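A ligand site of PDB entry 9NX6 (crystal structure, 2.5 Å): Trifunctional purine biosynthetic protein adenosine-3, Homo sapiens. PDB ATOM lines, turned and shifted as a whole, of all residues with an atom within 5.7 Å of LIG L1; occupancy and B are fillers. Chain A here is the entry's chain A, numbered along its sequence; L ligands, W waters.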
ATOM      1  N   GLY A  10     -28.713 -17.803 -11.653  1.00  0.00           N
ATOM      2  CA  GLY A  10     -27.515 -17.503 -10.895  1.00  0.00           C
ATOM      3  C   GLY A  10     -26.497 -16.615 -11.577  1.00  0.00           C
ATOM      4  O   GLY A  10     -26.839 -15.543 -12.080  1.00  0.00           O
ATOM      5  N   THR A  11     -25.235 -17.065 -11.580  1.00  0.00           N
ATOM      6  CA  THR A  11     -24.089 -16.248 -11.981  1.00  0.00           C
ATOM      7  C   THR A  11     -24.234 -15.695 -13.402  1.00  0.00           C
ATOM      8  O   THR A  11     -23.759 -14.583 -13.687  1.00  0.00           O
ATOM      9  CB  THR A  11     -22.805 -17.078 -11.890  1.00  0.00           C
ATOM     10  OG1 THR A  11     -22.613 -17.501 -10.533  1.00  0.00           O
ATOM     11  CG2 THR A  11     -21.607 -16.254 -12.339  1.00  0.00           C
ATOM     12  N   GLY A  12     -24.840 -16.463 -14.307  1.00  0.00           N
ATOM     13  CA  GLY A  12     -25.093 -15.947 -15.635  1.00  0.00           C
ATOM     14  C   GLY A  12     -23.914 -15.931 -16.589  1.00  0.00           C
ATOM     15  O   GLY A  12     -23.875 -15.080 -17.477  1.00  0.00           O
ATOM     16  N   SER A  13     -22.949 -16.838 -16.427  1.00  0.00           N
ATOM     17  CA  SER A  13     -21.829 -16.839 -17.343  1.00  0.00           C
ATOM     18  C   SER A  13     -22.228 -17.383 -18.723  1.00  0.00           C
ATOM     19  O   SER A  13     -21.662 -16.965 -19.732  1.00  0.00           O
ATOM     20  CB  SER A  13     -20.664 -17.632 -16.754  1.00  0.00           C
ATOM     21  OG  SER A  13     -20.838 -19.029 -16.843  1.00  0.00           O
ATOM     22  N   ASN A  14     -23.204 -18.295 -18.777  1.00  0.00           N
ATOM     23  CA  ASN A  14     -23.737 -18.670 -20.081  1.00  0.00           C
ATOM     24  C   ASN A  14     -24.503 -17.500 -20.696  1.00  0.00           C
ATOM     25  O   ASN A  14     -24.328 -17.195 -21.880  1.00  0.00           O
ATOM     26  CB  ASN A  14     -24.632 -19.903 -19.976  1.00  0.00           C
ATOM     27  CG  ASN A  14     -23.838 -21.179 -19.916  1.00  0.00           C
ATOM     28  OD1 ASN A  14     -23.268 -21.597 -20.915  1.00  0.00           O
ATOM     29  ND2 ASN A  14     -23.773 -21.777 -18.750  1.00  0.00           N
ATOM     30  N   LEU A  15     -25.313 -16.815 -19.888  1.00  0.00           N
ATOM     31  CA  LEU A  15     -25.946 -15.589 -20.332  1.00  0.00           C
ATOM     32  C   LEU A  15     -24.918 -14.655 -20.966  1.00  0.00           C
ATOM     33  O   LEU A  15     -25.127 -14.138 -22.069  1.00  0.00           O
ATOM     34  CB  LEU A  15     -26.640 -14.898 -19.176  1.00  0.00           C
ATOM     35  CG  LEU A  15     -27.200 -13.520 -19.576  1.00  0.00           C
ATOM     36  CD1 LEU A  15     -28.189 -13.693 -20.727  1.00  0.00           C
ATOM     37  CD2 LEU A  15     -27.849 -12.804 -18.411  1.00  0.00           C
ATOM     38  N   ALA A  87     -30.460 -20.815 -19.308  1.00  0.00           N
ATOM     39  CA  ALA A  87     -29.009 -20.694 -19.072  1.00  0.00           C
ATOM     40  C   ALA A  87     -28.757 -20.709 -17.568  1.00  0.00           C
ATOM     41  O   ALA A  87     -28.474 -19.680 -16.957  1.00  0.00           O
ATOM     42  CB  ALA A  87     -28.470 -19.422 -19.719  1.00  0.00           C
ATOM     43  N   GLY A  88     -28.828 -21.891 -16.970  1.00  0.00           N
ATOM     44  CA  GLY A  88     -28.714 -21.968 -15.539  1.00  0.00           C
ATOM     45  C   GLY A  88     -30.005 -21.746 -14.818  1.00  0.00           C
ATOM     46  O   GLY A  88     -29.993 -21.384 -13.636  1.00  0.00           O
ATOM     47  N   PHE A  89     -31.138 -21.948 -15.486  1.00  0.00           N
ATOM     48  CA  PHE A  89     -32.439 -21.859 -14.860  1.00  0.00           C
ATOM     49  C   PHE A  89     -32.661 -23.086 -13.984  1.00  0.00           C
ATOM     50  O   PHE A  89     -32.721 -24.203 -14.491  1.00  0.00           O
ATOM     51  CB  PHE A  89     -33.514 -21.766 -15.943  1.00  0.00           C
ATOM     52  CG  PHE A  89     -34.840 -21.324 -15.448  1.00  0.00           C
ATOM     53  CD1 PHE A  89     -34.993 -20.103 -14.833  1.00  0.00           C
ATOM     54  CD2 PHE A  89     -35.952 -22.157 -15.582  1.00  0.00           C
ATOM     55  CE1 PHE A  89     -36.225 -19.699 -14.358  1.00  0.00           C
ATOM     56  CE2 PHE A  89     -37.193 -21.752 -15.102  1.00  0.00           C
ATOM     57  CZ  PHE A  89     -37.336 -20.522 -14.491  1.00  0.00           C
ATOM     58  N   MET A  90     -32.783 -22.891 -12.685  1.00  0.00           N
ATOM     59  CA  MET A  90     -32.908 -24.038 -11.779  1.00  0.00           C
ATOM     60  C   MET A  90     -34.353 -24.246 -11.326  1.00  0.00           C
ATOM     61  O   MET A  90     -34.670 -24.307 -10.135  1.00  0.00           O
ATOM     62  CB  MET A  90     -31.993 -23.852 -10.576  1.00  0.00           C
ATOM     63  CG  MET A  90     -30.554 -23.811 -10.938  1.00  0.00           C
ATOM     64  SD  MET A  90     -30.151 -25.423 -11.605  1.00  0.00           S
ATOM     65  CE  MET A  90     -28.451 -25.194 -12.130  1.00  0.00           C
ATOM     66  N   ASN A 107     -31.888 -25.740 -23.686  1.00  0.00           N
ATOM     67  CA  ASN A 107     -31.304 -25.864 -22.361  1.00  0.00           C
ATOM     68  C   ASN A 107     -29.856 -26.283 -22.485  1.00  0.00           C
ATOM     69  O   ASN A 107     -29.509 -27.081 -23.359  1.00  0.00           O
ATOM     70  CB  ASN A 107     -32.063 -26.866 -21.541  1.00  0.00           C
ATOM     71  CG  ASN A 107     -31.484 -27.033 -20.169  1.00  0.00           C
ATOM     72  OD1 ASN A 107     -31.316 -26.062 -19.439  1.00  0.00           O
ATOM     73  ND2 ASN A 107     -31.187 -28.274 -19.792  1.00  0.00           N
ATOM     74  N   ILE A 108     -28.997 -25.727 -21.621  1.00  0.00           N
ATOM     75  CA  ILE A 108     -27.599 -26.167 -21.496  1.00  0.00           C
ATOM     76  C   ILE A 108     -27.491 -27.037 -20.250  1.00  0.00           C
ATOM     77  O   ILE A 108     -27.760 -26.574 -19.132  1.00  0.00           O
ATOM     78  CB  ILE A 108     -26.642 -24.983 -21.418  1.00  0.00           C
ATOM     79  CG1 ILE A 108     -25.211 -25.488 -21.275  1.00  0.00           C
ATOM     80  CG2 ILE A 108     -27.000 -24.093 -20.246  1.00  0.00           C
ATOM     81  CD1 ILE A 108     -24.749 -26.372 -22.384  1.00  0.00           C
ATOM     82  N   HIS A 109     -27.132 -28.305 -20.453  1.00  0.00           N
ATOM     83  CA  HIS A 109     -26.957 -29.250 -19.370  1.00  0.00           C
ATOM     84  C   HIS A 109     -25.497 -29.702 -19.313  1.00  0.00           C
ATOM     85  O   HIS A 109     -24.907 -30.018 -20.361  1.00  0.00           O
ATOM     86  CB  HIS A 109     -27.873 -30.450 -19.563  1.00  0.00           C
ATOM     87  CG  HIS A 109     -27.680 -31.525 -18.535  1.00  0.00           C
ATOM     88  ND1 HIS A 109     -28.214 -31.440 -17.263  1.00  0.00           N
ATOM     89  CD2 HIS A 109     -27.007 -32.701 -18.586  1.00  0.00           C
ATOM     90  CE1 HIS A 109     -27.884 -32.524 -16.583  1.00  0.00           C
ATOM     91  NE2 HIS A 109     -27.141 -33.295 -17.358  1.00  0.00           N
ATOM     92  N   PRO A 110     -24.886 -29.759 -18.131  1.00  0.00           N
ATOM     93  CA  PRO A 110     -23.431 -29.940 -18.046  1.00  0.00           C
ATOM     94  C   PRO A 110     -23.033 -31.410 -17.986  1.00  0.00           C
ATOM     95  O   PRO A 110     -22.254 -31.833 -17.135  1.00  0.00           O
ATOM     96  CB  PRO A 110     -23.067 -29.196 -16.750  1.00  0.00           C
ATOM     97  CG  PRO A 110     -24.332 -29.349 -15.876  1.00  0.00           C
ATOM     98  CD  PRO A 110     -25.491 -29.772 -16.799  1.00  0.00           C
ATOM     99  N   GLY A 118     -30.257 -34.801 -14.631  1.00  0.00           N
ATOM    100  CA  GLY A 118     -30.536 -34.322 -13.298  1.00  0.00           C
ATOM    101  C   GLY A 118     -29.628 -33.175 -12.900  1.00  0.00           C
ATOM    102  O   GLY A 118     -28.855 -32.629 -13.704  1.00  0.00           O
ATOM    103  N   SER A 119     -29.739 -32.798 -11.634  1.00  0.00           N
ATOM    104  CA  SER A 119     -29.235 -31.493 -11.233  1.00  0.00           C
ATOM    105  C   SER A 119     -27.793 -31.509 -10.754  1.00  0.00           C
ATOM    106  O   SER A 119     -27.133 -30.470 -10.798  1.00  0.00           O
ATOM    107  CB  SER A 119     -30.131 -30.910 -10.137  1.00  0.00           C
ATOM    108  OG  SER A 119     -30.309 -31.859  -9.109  1.00  0.00           O
ATOM    109  N   HIS A 122     -22.158 -32.966 -12.429  1.00  0.00           N
ATOM    110  CA  HIS A 122     -20.735 -33.079 -12.131  1.00  0.00           C
ATOM    111  C   HIS A 122     -20.477 -34.057 -10.977  1.00  0.00           C
ATOM    112  O   HIS A 122     -19.509 -34.829 -11.016  1.00  0.00           O
ATOM    113  CB  HIS A 122     -20.167 -31.704 -11.802  1.00  0.00           C
ATOM    114  CG  HIS A 122     -20.153 -30.761 -12.963  1.00  0.00           C
ATOM    115  ND1 HIS A 122     -19.640 -31.098 -14.193  1.00  0.00           N
ATOM    116  CD2 HIS A 122     -20.611 -29.492 -13.082  1.00  0.00           C
ATOM    117  CE1 HIS A 122     -19.768 -30.084 -15.018  1.00  0.00           C
ATOM    118  NE2 HIS A 122     -20.356 -29.087 -14.368  1.00  0.00           N
ATOM    119  N   ASP A 145     -34.084 -33.204 -19.277  1.00  0.00           N
ATOM    120  CA  ASP A 145     -32.848 -33.573 -19.980  1.00  0.00           C
ATOM    121  C   ASP A 145     -33.065 -34.735 -20.945  1.00  0.00           C
ATOM    122  O   ASP A 145     -32.273 -35.681 -20.998  1.00  0.00           O
ATOM    123  CB  ASP A 145     -31.720 -33.885 -18.999  1.00  0.00           C
ATOM    124  CG  ASP A 145     -31.586 -32.855 -17.898  1.00  0.00           C
ATOM    125  OD1 ASP A 145     -31.667 -31.639 -18.206  1.00  0.00           O
ATOM    126  OD2 ASP A 145     -31.422 -33.262 -16.726  1.00  0.00           O
ATOM    127  N   SER A 167     -16.500 -28.292 -13.267  1.00  0.00           N
ATOM    128  CA  SER A 167     -17.477 -27.385 -13.872  1.00  0.00           C
ATOM    129  C   SER A 167     -16.844 -26.129 -14.415  1.00  0.00           C
ATOM    130  O   SER A 167     -17.441 -25.472 -15.262  1.00  0.00           O
ATOM    131  CB  SER A 167     -18.557 -27.000 -12.871  1.00  0.00           C
ATOM    132  OG  SER A 167     -17.963 -26.573 -11.675  1.00  0.00           O
ATOM    133  N   LYS A 171     -17.635 -25.437 -18.333  1.00  0.00           N
ATOM    134  CA  LYS A 171     -18.283 -24.176 -18.676  1.00  0.00           C
ATOM    135  C   LYS A 171     -17.627 -23.482 -19.856  1.00  0.00           C
ATOM    136  O   LYS A 171     -18.295 -22.746 -20.583  1.00  0.00           O
ATOM    137  CB  LYS A 171     -18.291 -23.251 -17.456  1.00  0.00           C
ATOM    138  CG  LYS A 171     -19.498 -23.412 -16.551  1.00  0.00           C
ATOM    139  CD  LYS A 171     -19.302 -22.568 -15.310  1.00  0.00           C
ATOM    140  CE  LYS A 171     -20.247 -22.949 -14.185  1.00  0.00           C
ATOM    141  NZ  LYS A 171     -21.385 -21.989 -14.017  1.00  0.00           N
ATOM    142  N   GLU A 174     -19.370 -24.960 -22.537  1.00  0.00           N
ATOM    143  CA  GLU A 174     -20.731 -24.457 -22.594  1.00  0.00           C
ATOM    144  C   GLU A 174     -20.797 -23.114 -23.297  1.00  0.00           C
ATOM    145  O   GLU A 174     -21.682 -22.876 -24.112  1.00  0.00           O
ATOM    146  CB  GLU A 174     -21.318 -24.367 -21.189  1.00  0.00           C
ATOM    147  CG  GLU A 174     -21.364 -25.688 -20.493  1.00  0.00           C
ATOM    148  CD  GLU A 174     -21.912 -25.562 -19.085  1.00  0.00           C
ATOM    149  OE1 GLU A 174     -21.890 -26.551 -18.330  1.00  0.00           O
ATOM    150  OE2 GLU A 174     -22.387 -24.454 -18.739  1.00  0.00           O
ATOM    151  N   HIS A 175     -19.855 -22.216 -22.991  1.00  0.00           N
ATOM    152  CA  HIS A 175     -19.812 -20.908 -23.639  1.00  0.00           C
ATOM    153  C   HIS A 175     -19.485 -20.989 -25.123  1.00  0.00           C
ATOM    154  O   HIS A 175     -19.587 -19.976 -25.820  1.00  0.00           O
ATOM    155  CB  HIS A 175     -18.784 -20.036 -22.921  1.00  0.00           C
ATOM    156  CG  HIS A 175     -19.051 -19.899 -21.459  1.00  0.00           C
ATOM    157  ND1 HIS A 175     -18.070 -19.558 -20.560  1.00  0.00           N
ATOM    158  CD2 HIS A 175     -20.183 -20.094 -20.742  1.00  0.00           C
ATOM    159  CE1 HIS A 175     -18.593 -19.532 -19.340  1.00  0.00           C
ATOM    160  NE2 HIS A 175     -19.876 -19.839 -19.423  1.00  0.00           N
HETATM  161  C1  LIG L   1     -24.165 -24.218 -16.071  1.00  0.00           C
HETATM  162  O1  LIG L   1     -22.901 -24.752 -15.710  1.00  0.00           O
HETATM  163  C2  LIG L   1     -25.093 -25.338 -16.537  1.00  0.00           C
HETATM  164  O2  LIG L   1     -24.412 -26.448 -17.131  1.00  0.00           O
HETATM  165  C3  LIG L   1     -25.799 -25.682 -15.241  1.00  0.00           C
HETATM  166  O3  LIG L   1     -25.754 -24.515 -14.402  1.00  0.00           O
HETATM  167  C4  LIG L   1     -24.729 -23.588 -14.793  1.00  0.00           C
HETATM  168  C5  LIG L   1     -25.206 -22.156 -14.914  1.00  0.00           C
HETATM  169  O4  LIG L   1     -24.005 -21.376 -14.860  1.00  0.00           O
HETATM  170  N1  LIG L   1     -27.180 -26.114 -15.298  1.00  0.00           N
HETATM  171  C6  LIG L   1     -27.516 -27.254 -14.649  1.00  0.00           C
HETATM  172  O5  LIG L   1     -26.760 -27.861 -13.855  1.00  0.00           O
HETATM  173  C7  LIG L   1     -28.911 -27.744 -15.007  1.00  0.00           C
HETATM  174  N2  LIG L   1     -29.244 -29.041 -14.429  1.00  0.00           N
HETATM  175  P1  LIG L   1     -24.065 -19.834 -15.249  1.00  0.00           P
HETATM  176  O6  LIG L   1     -22.703 -19.279 -14.908  1.00  0.00           O
HETATM  177  O7  LIG L   1     -24.398 -19.882 -16.743  1.00  0.00           O
HETATM  178  O8  LIG L   1     -25.162 -19.309 -14.353  1.00  0.00           O
HETATM  179  C1  LG2 L   2     -33.884 -28.399 -11.738  1.00  0.00           C
HETATM  180  C2  LG2 L   2     -34.427 -29.261 -10.754  1.00  0.00           C
HETATM  181  C3  LG2 L   2     -32.882 -30.425 -12.475  1.00  0.00           C
HETATM  182  C4  LG2 L   2     -33.044 -29.047 -12.683  1.00  0.00           C
HETATM  183  C5  LG2 L   2     -36.259 -25.818  -7.799  1.00  0.00           C
HETATM  184  C6  LG2 L   2     -35.021 -25.863  -6.906  1.00  0.00           C
HETATM  185  C7  LG2 L   2     -35.377 -28.907  -9.615  1.00  0.00           C
HETATM  186  C8  LG2 L   2     -34.830 -24.519  -6.204  1.00  0.00           C
HETATM  187  N1  LG2 L   2     -40.084 -30.045 -18.287  1.00  0.00           N
HETATM  188  C9  LG2 L   2     -36.689 -27.170  -8.353  1.00  0.00           C
HETATM  189  C10 LG2 L   2     -38.701 -29.669 -18.311  1.00  0.00           C
HETATM  190  C11 LG2 L   2     -36.562 -30.015 -19.113  1.00  0.00           C
HETATM  191  C12 LG2 L   2     -34.739 -28.391 -18.240  1.00  0.00           C
HETATM  192  C13 LG2 L   2     -34.601 -27.284 -17.387  1.00  0.00           C
HETATM  193  C14 LG2 L   2     -36.101 -28.922 -18.335  1.00  0.00           C
HETATM  194  C15 LG2 L   2     -37.032 -28.224 -17.564  1.00  0.00           C
HETATM  195  C16 LG2 L   2     -38.091 -27.008  -8.962  1.00  0.00           C
HETATM  196  C17 LG2 L   2     -33.340 -26.497 -17.068  1.00  0.00           C
HETATM  197  C18 LG2 L   2     -32.456 -27.280 -16.093  1.00  0.00           C
HETATM  198  C19 LG2 L   2     -33.263 -27.906 -14.961  1.00  0.00           C
HETATM  199  C20 LG2 L   2     -32.354 -28.270 -13.801  1.00  0.00           C
HETATM  200  F1  LG2 L   2     -34.140 -27.064 -11.778  1.00  0.00           F
HETATM  201  N2  LG2 L   2     -38.317 -28.627 -17.573  1.00  0.00           N
HETATM  202  N3  LG2 L   2     -37.851 -30.370 -19.076  1.00  0.00           N
HETATM  203  N4  LG2 L   2     -35.777 -27.525  -9.406  1.00  0.00           N
HETATM  204  O1  LG2 L   2     -35.785 -30.615 -19.779  1.00  0.00           O
HETATM  205  O2  LG2 L   2     -35.795 -29.752  -8.908  1.00  0.00           O
HETATM  206  O3  LG2 L   2     -34.280 -24.477  -5.064  1.00  0.00           O
HETATM  207  O4  LG2 L   2     -35.220 -23.449  -6.759  1.00  0.00           O
HETATM  208  O5  LG2 L   2     -39.073 -26.858  -8.192  1.00  0.00           O
HETATM  209  O6  LG2 L   2     -38.254 -27.009 -10.212  1.00  0.00           O
HETATM  210  S1  LG2 L   2     -36.146 -26.969 -16.797  1.00  0.00           S
HETATM  211  S2  LG2 L   2     -33.820 -30.783 -11.109  1.00  0.00           S
HETATM  212  O   HOH W   1     -30.344 -29.608 -17.172  1.00  0.00           O
HETATM  213  O   HOH W   2     -24.816 -19.745 -11.972  1.00  0.00           O
HETATM  214  O   HOH W   3     -20.374 -26.539 -15.686  1.00  0.00           O
HETATM  215  O   HOH W   4     -26.734 -30.858 -13.488  1.00  0.00           O
HETATM  216  O   HOH W   5     -32.030 -30.923 -15.061  1.00  0.00           O
HETATM  217  O   HOH W   6     -22.097 -26.266 -13.792  1.00  0.00           O
HETATM  218  O   HOH W   7     -27.808 -18.667 -13.959  1.00  0.00           O
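Water W2 bridges an oxygen (O8) of LIG L1 and the backbone NH (N) of Thr 11. Water W6 bridges an oxygen (O1) of LIG L1 (2.6 Å) and a ring nitrogen (NE2) of His 122 (3.4 Å). Water W7 lies within hydrogen-bond range of N of Gly 10 (2.6 Å), O8 of LIG L1 (2.8 Å) and O of Ala 87 (3.2 Å). Water W1 lies within hydrogen-bond range of the side-chain carboxylate of Asp 145 (2.6 Å), a ring nitrogen (ND1) of His 109 (2.8 Å), a nitrogen (N2) of LIG L1 (3.0 Å) and the side-chain amide nitrogen of Asn 107 (3.1 Å). Water W3 lies within hydrogen-bond range of NE2 of His 122, OE1 of Glu 174, O1 of LIG L1 and O of Ser 167. Water W5 lies within hydrogen-bond range of the side-chain carboxylate (OD2) of Asp 145 and a nitrogen (N2) of LIG L1.
The side-chain hydroxyl of Ser 13 sits at hydrogen-bond distance from an oxygen (O6) of LIG L1 (2.7 Å). O6 of LIG L1 lies within hydrogen-bond range of N of Ser 13 (2.9 Å). An oxygen (O6) of LIG L1 is in salt-bridge range of the side-chain amino group (NZ) of Lys 171, at 3.1 Å. O8 of LIG L1 lies within hydrogen-bond range of N of Gly 12, at 2.9 Å. The backbone carbonyl oxygen of Met 90 sits close to a nitrogen (N4) of LG2 L2, 3.5 Å away. The backbone NH (N) of Asn 14 sits at hydrogen-bond distance from an oxygen (O7) of LIG L1 (2.8 Å). N of Asp 145 sits at hydrogen-bond distance from O1 of LG2 L2, at 3.1 Å. The side-chain carboxylate (OE1) of Glu 174 is in hydrogen-bond range of an oxygen (O2) of LIG L1 (2.8 Å). An oxygen (O7) of LIG L1 sits at hydrogen-bond distance from the side-chain amide nitrogen of Asn 14, 2.8 Å away.
The side-chain hydroxyl (OG) of Ser 13 sits at hydrogen-bond distance from a ring nitrogen (NE2) of His 175 (2.9 Å). ND1 of His 175 lies close to O of Lys 171, 3.2 Å away. The side-chain carboxylate (OE2) of Glu 174 is in hydrogen-bond range of the side-chain amide nitrogen (ND2) of Asn 14 (3.0 Å). The backbone NH (N) of Gly 118 is in hydrogen-bond range of the side-chain carboxylate (OD2) of Asp 145.
O2 of LIG L1 lies close to N of Pro 110 (3.5 Å). Thr 11 touches LIG L1 (N to O8, 3.6 Å). Gly 88 touches LIG L1 (CA to C5, 3.6 Å). Met 90 touches LIG L1. Ile 108 touches LIG L1. ND1 of His 109 touches N2 of LIG L1, 3.9 Å away. O of Gly 118 touches N2 of LIG L1, 3.7 Å away. Hydrophobic or aromatic side chains that line LIG L1: Met 90 and Pro 110. Of the 22 residues printed, 12 come within 4 Å of LIG L1. The nearest printed residue that does not touch LIG L1 is Ser 119 (4.03 Å).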
